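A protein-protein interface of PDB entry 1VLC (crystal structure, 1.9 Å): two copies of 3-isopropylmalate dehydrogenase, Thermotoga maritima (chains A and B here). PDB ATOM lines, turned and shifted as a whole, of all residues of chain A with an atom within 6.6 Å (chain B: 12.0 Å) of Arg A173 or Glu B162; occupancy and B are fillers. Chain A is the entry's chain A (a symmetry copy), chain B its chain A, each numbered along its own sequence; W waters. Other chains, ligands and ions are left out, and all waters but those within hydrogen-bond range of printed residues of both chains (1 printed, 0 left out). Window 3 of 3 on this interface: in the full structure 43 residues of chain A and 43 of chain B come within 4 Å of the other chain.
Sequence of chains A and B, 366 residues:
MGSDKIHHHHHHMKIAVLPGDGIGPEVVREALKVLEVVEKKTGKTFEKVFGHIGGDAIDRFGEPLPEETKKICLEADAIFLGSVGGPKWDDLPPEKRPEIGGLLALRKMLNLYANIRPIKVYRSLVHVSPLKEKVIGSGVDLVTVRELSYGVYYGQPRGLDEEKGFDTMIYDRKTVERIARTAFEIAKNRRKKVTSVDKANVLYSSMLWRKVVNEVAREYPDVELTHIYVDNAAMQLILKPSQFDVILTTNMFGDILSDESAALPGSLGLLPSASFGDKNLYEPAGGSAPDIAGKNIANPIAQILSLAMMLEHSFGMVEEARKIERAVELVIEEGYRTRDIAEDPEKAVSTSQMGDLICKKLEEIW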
ATOM      1  N   TYR A 171      13.253  -9.978  21.253  1.00  0.00           N
ATOM      2  CA  TYR A 171      14.573  -9.373  20.996  1.00  0.00           C
ATOM      3  C   TYR A 171      15.478 -10.428  20.415  1.00  0.00           C
ATOM      4  O   TYR A 171      15.314 -11.651  20.723  1.00  0.00           O
ATOM      5  CB  TYR A 171      15.169  -8.735  22.252  1.00  0.00           C
ATOM      6  CG  TYR A 171      14.627  -7.380  22.450  1.00  0.00           C
ATOM      7  CD1 TYR A 171      15.069  -6.325  21.660  1.00  0.00           C
ATOM      8  CD2 TYR A 171      13.624  -7.116  23.419  1.00  0.00           C
ATOM      9  CE1 TYR A 171      14.494  -5.069  21.754  1.00  0.00           C
ATOM     10  CE2 TYR A 171      13.057  -5.798  23.509  1.00  0.00           C
ATOM     11  CZ  TYR A 171      13.562  -4.787  22.715  1.00  0.00           C
ATOM     12  OH  TYR A 171      13.048  -3.496  22.698  1.00  0.00           O
ATOM     13  N   ASP A 172      16.345  -9.964  19.503  1.00  0.00           N
ATOM     14  CA  ASP A 172      17.399 -10.740  18.970  1.00  0.00           C
ATOM     15  C   ASP A 172      18.722 -10.089  19.226  1.00  0.00           C
ATOM     16  O   ASP A 172      18.787  -8.908  19.589  1.00  0.00           O
ATOM     17  CB  ASP A 172      17.205 -11.049  17.504  1.00  0.00           C
ATOM     18  CG  ASP A 172      16.973  -9.862  16.658  1.00  0.00           C
ATOM     19  OD1 ASP A 172      17.483  -8.758  16.958  1.00  0.00           O
ATOM     20  OD2 ASP A 172      16.317  -9.999  15.591  1.00  0.00           O
ATOM     21  N   ARG A 173      19.779 -10.860  19.004  1.00  0.00           N
ATOM     22  CA  ARG A 173      21.124 -10.408  19.306  1.00  0.00           C
ATOM     23  C   ARG A 173      21.482  -9.104  18.632  1.00  0.00           C
ATOM     24  O   ARG A 173      21.985  -8.212  19.295  1.00  0.00           O
ATOM     25  CB  ARG A 173      22.173 -11.494  18.992  1.00  0.00           C
ATOM     26  CG  ARG A 173      23.635 -11.004  19.138  1.00  0.00           C
ATOM     27  CD  ARG A 173      24.731 -12.144  19.112  1.00  0.00           C
ATOM     28  NE  ARG A 173      24.741 -12.863  20.394  1.00  0.00           N
ATOM     29  CZ  ARG A 173      24.122 -14.011  20.599  1.00  0.00           C
ATOM     30  NH1 ARG A 173      23.457 -14.595  19.609  1.00  0.00           N
ATOM     31  NH2 ARG A 173      24.138 -14.572  21.804  1.00  0.00           N
ATOM     32  N   LYS A 174      21.270  -8.985  17.318  1.00  0.00           N
ATOM     33  CA  LYS A 174      21.709  -7.789  16.613  1.00  0.00           C
ATOM     34  C   LYS A 174      21.056  -6.535  17.120  1.00  0.00           C
ATOM     35  O   LYS A 174      21.683  -5.465  17.196  1.00  0.00           O
ATOM     36  CB  LYS A 174      21.542  -7.945  15.093  1.00  0.00           C
ATOM     37  CG  LYS A 174      20.084  -8.013  14.637  1.00  0.00           C
ATOM     38  CD  LYS A 174      19.935  -8.376  13.139  1.00  0.00           C
ATOM     39  CE  LYS A 174      18.438  -8.430  12.702  1.00  0.00           C
ATOM     40  NZ  LYS A 174      18.271  -9.046  11.315  1.00  0.00           N
ATOM     41  N   THR A 175      19.784  -6.644  17.490  1.00  0.00           N
ATOM     42  CA  THR A 175      19.042  -5.507  18.027  1.00  0.00           C
ATOM     43  C   THR A 175      19.617  -5.088  19.366  1.00  0.00           C
ATOM     44  O   THR A 175      19.879  -3.915  19.566  1.00  0.00           O
ATOM     45  CB  THR A 175      17.525  -5.868  18.193  1.00  0.00           C
ATOM     46  OG1 THR A 175      16.999  -6.245  16.916  1.00  0.00           O
ATOM     47  CG2 THR A 175      16.748  -4.678  18.624  1.00  0.00           C
ATOM     48  N   VAL A 176      19.870  -6.047  20.253  1.00  0.00           N
ATOM     49  CA  VAL A 176      20.325  -5.723  21.593  1.00  0.00           C
ATOM     50  C   VAL A 176      21.765  -5.220  21.506  1.00  0.00           C
ATOM     51  O   VAL A 176      22.106  -4.303  22.163  1.00  0.00           O
ATOM     52  CB  VAL A 176      20.213  -6.949  22.527  1.00  0.00           C
ATOM     53  CG1 VAL A 176      20.751  -6.587  23.895  1.00  0.00           C
ATOM     54  CG2 VAL A 176      18.782  -7.341  22.617  1.00  0.00           C
ATOM     55  N   GLU A 177      22.592  -5.811  20.655  1.00  0.00           N
ATOM     56  CA  GLU A 177      23.993  -5.305  20.464  1.00  0.00           C
ATOM     57  C   GLU A 177      24.000  -3.825  20.151  1.00  0.00           C
ATOM     58  O   GLU A 177      24.761  -3.053  20.707  1.00  0.00           O
ATOM     59  CB  GLU A 177      24.680  -6.048  19.330  1.00  0.00           C
ATOM     60  CG  GLU A 177      25.223  -7.400  19.684  1.00  0.00           C
ATOM     61  CD  GLU A 177      25.762  -8.204  18.477  1.00  0.00           C
ATOM     62  OE1 GLU A 177      25.590  -7.781  17.305  1.00  0.00           O
ATOM     63  OE2 GLU A 177      26.340  -9.294  18.728  1.00  0.00           O
ATOM     64  N   ARG A 178      23.144  -3.404  19.221  1.00  0.00           N
ATOM     65  CA  ARG A 178      23.146  -2.041  18.767  1.00  0.00           C
ATOM     66  C   ARG A 178      22.820  -1.059  19.885  1.00  0.00           C
ATOM     67  O   ARG A 178      23.500  -0.071  20.067  1.00  0.00           O
ATOM     68  CB  ARG A 178      22.154  -1.912  17.613  1.00  0.00           C
ATOM     69  CG  ARG A 178      22.151  -0.551  16.871  1.00  0.00           C
ATOM     70  CD  ARG A 178      20.937  -0.466  16.030  1.00  0.00           C
ATOM     71  NE  ARG A 178      21.171   0.353  14.888  1.00  0.00           N
ATOM     72  CZ  ARG A 178      20.278   0.552  13.944  1.00  0.00           C
ATOM     73  NH1 ARG A 178      19.080  -0.075  13.978  1.00  0.00           N
ATOM     74  NH2 ARG A 178      20.607   1.360  12.948  1.00  0.00           N
ATOM     75  N   LEU A 208      17.360 -13.194  26.807  1.00  0.00           N
ATOM     76  CA  LEU A 208      18.246 -12.897  25.639  1.00  0.00           C
ATOM     77  C   LEU A 208      18.899 -11.517  25.810  1.00  0.00           C
ATOM     78  O   LEU A 208      20.112 -11.389  25.719  1.00  0.00           O
ATOM     79  CB  LEU A 208      17.439 -12.963  24.350  1.00  0.00           C
ATOM     80  CG  LEU A 208      18.066 -12.723  22.969  1.00  0.00           C
ATOM     81  CD1 LEU A 208      18.407 -11.281  22.681  1.00  0.00           C
ATOM     82  CD2 LEU A 208      19.279 -13.604  22.869  1.00  0.00           C
ATOM     83  N   LYS A 211      21.733 -11.609  28.400  1.00  0.00           N
ATOM     84  CA  LYS A 211      22.854 -12.399  27.844  1.00  0.00           C
ATOM     85  C   LYS A 211      23.648 -11.555  26.906  1.00  0.00           C
ATOM     86  O   LYS A 211      24.843 -11.440  27.114  1.00  0.00           O
ATOM     87  CB  LYS A 211      22.338 -13.662  27.166  1.00  0.00           C
ATOM     88  CG  LYS A 211      23.369 -14.569  26.477  1.00  0.00           C
ATOM     89  CD  LYS A 211      22.706 -15.903  26.026  1.00  0.00           C
ATOM     90  CE  LYS A 211      21.780 -15.808  24.768  1.00  0.00           C
ATOM     91  NZ  LYS A 211      20.732 -16.947  24.610  1.00  0.00           N
ATOM     92  N   VAL A 212      22.993 -10.872  25.943  1.00  0.00           N
ATOM     93  CA  VAL A 212      23.712 -10.023  24.987  1.00  0.00           C
ATOM     94  C   VAL A 212      24.291  -8.762  25.587  1.00  0.00           C
ATOM     95  O   VAL A 212      25.359  -8.364  25.240  1.00  0.00           O
ATOM     96  CB  VAL A 212      22.831  -9.695  23.829  1.00  0.00           C
ATOM     97  CG1 VAL A 212      23.536  -8.835  22.845  1.00  0.00           C
ATOM     98  CG2 VAL A 212      22.368 -11.027  23.201  1.00  0.00           C
ATOM     99  N   GLU A 215      27.480  -9.768  27.150  1.00  0.00           N
ATOM    100  CA  GLU A 215      28.472  -9.890  26.075  1.00  0.00           C
ATOM    101  C   GLU A 215      29.057  -8.581  25.635  1.00  0.00           C
ATOM    102  O   GLU A 215      30.270  -8.444  25.524  1.00  0.00           O
ATOM    103  CB  GLU A 215      27.886 -10.538  24.834  1.00  0.00           C
ATOM    104  CG  GLU A 215      27.726 -12.033  24.887  1.00  0.00           C
ATOM    105  CD  GLU A 215      26.736 -12.556  23.830  1.00  0.00           C
ATOM    106  OE1 GLU A 215      26.340 -11.797  22.908  1.00  0.00           O
ATOM    107  OE2 GLU A 215      26.307 -13.730  23.943  1.00  0.00           O
ATOM    108  N   ARG B 158       6.206 -19.070  23.298  1.00  0.00           N
ATOM    109  CA  ARG B 158       7.270 -18.369  23.973  1.00  0.00           C
ATOM    110  C   ARG B 158       8.511 -19.215  23.907  1.00  0.00           C
ATOM    111  O   ARG B 158       8.433 -20.432  23.755  1.00  0.00           O
ATOM    112  CB  ARG B 158       6.888 -17.973  25.406  1.00  0.00           C
ATOM    113  CG  ARG B 158       6.526 -19.096  26.337  1.00  0.00           C
ATOM    114  CD  ARG B 158       5.813 -18.666  27.591  1.00  0.00           C
ATOM    115  NE  ARG B 158       6.378 -17.417  28.082  1.00  0.00           N
ATOM    116  CZ  ARG B 158       7.117 -17.256  29.158  1.00  0.00           C
ATOM    117  NH1 ARG B 158       7.378 -18.268  29.984  1.00  0.00           N
ATOM    118  NH2 ARG B 158       7.586 -16.044  29.427  1.00  0.00           N
ATOM    119  N   GLY B 159       9.679 -18.612  23.986  1.00  0.00           N
ATOM    120  CA  GLY B 159      10.857 -19.425  23.836  1.00  0.00           C
ATOM    121  C   GLY B 159      12.115 -18.668  23.714  1.00  0.00           C
ATOM    122  O   GLY B 159      12.098 -17.450  23.522  1.00  0.00           O
ATOM    123  N   LEU B 160      13.224 -19.409  23.779  1.00  0.00           N
ATOM    124  CA  LEU B 160      14.563 -18.841  23.683  1.00  0.00           C
ATOM    125  C   LEU B 160      15.453 -19.739  22.888  1.00  0.00           C
ATOM    126  O   LEU B 160      15.498 -20.958  23.150  1.00  0.00           O
ATOM    127  CB  LEU B 160      15.116 -18.747  25.093  1.00  0.00           C
ATOM    128  CG  LEU B 160      16.501 -18.131  25.301  1.00  0.00           C
ATOM    129  CD1 LEU B 160      16.515 -16.642  25.009  1.00  0.00           C
ATOM    130  CD2 LEU B 160      16.916 -18.406  26.723  1.00  0.00           C
ATOM    131  N   ASP B 161      16.162 -19.197  21.934  1.00  0.00           N
ATOM    132  CA  ASP B 161      17.204 -19.954  21.305  1.00  0.00           C
ATOM    133  C   ASP B 161      18.462 -19.143  21.404  1.00  0.00           C
ATOM    134  O   ASP B 161      18.518 -18.208  22.197  1.00  0.00           O
ATOM    135  CB  ASP B 161      16.831 -20.348  19.881  1.00  0.00           C
ATOM    136  CG  ASP B 161      16.678 -19.170  18.952  1.00  0.00           C
ATOM    137  OD1 ASP B 161      17.522 -18.243  18.980  1.00  0.00           O
ATOM    138  OD2 ASP B 161      15.739 -19.118  18.128  1.00  0.00           O
ATOM    139  N   GLU B 162      19.472 -19.471  20.602  1.00  0.00           N
ATOM    140  CA  GLU B 162      20.745 -18.790  20.719  1.00  0.00           C
ATOM    141  C   GLU B 162      20.671 -17.344  20.242  1.00  0.00           C
ATOM    142  O   GLU B 162      21.405 -16.500  20.784  1.00  0.00           O
ATOM    143  CB  GLU B 162      21.848 -19.515  19.947  1.00  0.00           C
ATOM    144  N   GLU B 163      19.849 -17.039  19.238  1.00  0.00           N
ATOM    145  CA  GLU B 163      19.844 -15.651  18.719  1.00  0.00           C
ATOM    146  C   GLU B 163      18.636 -14.786  19.133  1.00  0.00           C
ATOM    147  O   GLU B 163      18.690 -13.594  18.948  1.00  0.00           O
ATOM    148  CB  GLU B 163      19.987 -15.620  17.188  1.00  0.00           C
ATOM    149  CG  GLU B 163      18.751 -16.089  16.423  1.00  0.00           C
ATOM    150  CD  GLU B 163      17.999 -14.965  15.699  1.00  0.00           C
ATOM    151  OE1 GLU B 163      18.126 -13.785  16.115  1.00  0.00           O
ATOM    152  OE2 GLU B 163      17.269 -15.264  14.712  1.00  0.00           O
ATOM    153  N   LYS B 164      17.575 -15.375  19.682  1.00  0.00           N
ATOM    154  CA  LYS B 164      16.394 -14.594  19.968  1.00  0.00           C
ATOM    155  C   LYS B 164      15.635 -15.165  21.135  1.00  0.00           C
ATOM    156  O   LYS B 164      15.662 -16.377  21.391  1.00  0.00           O
ATOM    157  CB  LYS B 164      15.520 -14.492  18.717  1.00  0.00           C
ATOM    158  CG  LYS B 164      14.716 -15.723  18.377  1.00  0.00           C
ATOM    159  CD  LYS B 164      14.006 -15.473  17.053  1.00  0.00           C
ATOM    160  N   GLY B 165      14.987 -14.296  21.873  1.00  0.00           N
ATOM    161  CA  GLY B 165      13.969 -14.714  22.818  1.00  0.00           C
ATOM    162  C   GLY B 165      12.672 -13.953  22.624  1.00  0.00           C
ATOM    163  O   GLY B 165      12.701 -12.764  22.343  1.00  0.00           O
ATOM    164  N   PHE B 166      11.557 -14.636  22.879  1.00  0.00           N
ATOM    165  CA  PHE B 166      10.238 -14.102  22.687  1.00  0.00           C
ATOM    166  C   PHE B 166       9.237 -14.641  23.646  1.00  0.00           C
ATOM    167  O   PHE B 166       9.320 -15.772  24.112  1.00  0.00           O
ATOM    168  CB  PHE B 166       9.673 -14.342  21.261  1.00  0.00           C
ATOM    169  CG  PHE B 166       9.488 -15.787  20.890  1.00  0.00           C
ATOM    170  CD1 PHE B 166      10.575 -16.568  20.562  1.00  0.00           C
ATOM    171  CD2 PHE B 166       8.214 -16.356  20.832  1.00  0.00           C
ATOM    172  CE1 PHE B 166      10.416 -17.921  20.198  1.00  0.00           C
ATOM    173  CE2 PHE B 166       8.035 -17.702  20.474  1.00  0.00           C
ATOM    174  CZ  PHE B 166       9.137 -18.486  20.151  1.00  0.00           C
HETATM  175  O   HOH W   1      20.097 -11.409  15.682  1.00  0.00           O
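Among the printed residues, pairs that only touch across the chains: Asp A172 with Glu B163, Tyr A171 with Lys B164, Lys A211 with Asp B161, Leu A208 with Gly B165, Leu A208 with Leu B160, Leu A208 with Lys B164, Lys A211 with Glu B162 and Leu A208 with Glu B163.
Of the printed residues of chain B, Arg A173 touches Glu B162 and Glu B163.
Of chain A, only Arg A173 and Lys A211 come within 4 Å of Glu B162.
Thr A175 touches none of the printed residues of chain B.
Val A176 touches none of the printed residues of chain B.
No residue of chain B comes within 4 Å of Glu A177.
Of chain B, only Asp B161 (3.5 Å) and Glu B162 (3.9 Å) come within 4 Å of Lys A211.
No residue of chain B comes within 4 Å of Val A212.
Of the printed residues of chain A, Lys B164 touches Tyr A171 (3.2 Å) and Leu A208 (3.9 Å).
Of the printed residues of chain A, Leu B160 touches Leu A208 (3.9 Å).
Printed residues of chain A within 4 Å of Gly B165: Tyr A171 and Leu A208.
Lys A174 touches none of the printed residues of chain B.
Arg A178 touches none of the printed residues of chain B.
The nearest printed residue of chain A that does not touch Lys B164 is Asp A172 (4.02 Å).
Water W1 lies within hydrogen-bond range of OE1 of Glu B163 (3.1 Å), N of Lys A174 (3.2 Å) and N of Arg A173 (3.4 Å).
Of the 12 printed residues of chain A, 5 touch a printed residue of chain B.
Hydrophobic or aromatic side chains of chain A that line the printed part of chain B: Leu A208.
Of the 9 printed residues of chain B, 6 touch a printed residue of chain A.
Among the printed residues, 11 pairs touch across the chains.
Among the printed residues, no Asp or Glu carboxylate lies within 4 Å of a Lys or Arg side-chain nitrogen of the other chain.
The backbone NH of Glu B163 is in hydrogen-bond range of the side-chain carboxylate of Asp B161 (2.6 Å).
The backbone NH (N) of Lys B164 sits at hydrogen-bond distance from the side-chain carboxylate (OD1) of Asp B161 (3.0 Å).
OD1 of Asp A172 is in hydrogen-bond range of OG1 of Thr A175 (2.6 Å).
The side-chain carboxylate (OE2) of Glu A215 lies within salt-bridge range of the guanidinium group (NH2) of Arg A173 (3.2 Å).
No position is printed for both chains.
Of the 11 pairs that touch across the chains among the printed residues, none has its exchanged pair printed and touching as well.
O of Glu B162 is in hydrogen-bond range of NH1 of Arg A173.
N of Arg A173 lies within hydrogen-bond range of O of Glu B163 (2.9 Å).
N of Gly B165 lies within hydrogen-bond range of O of Tyr A171 (2.9 Å).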
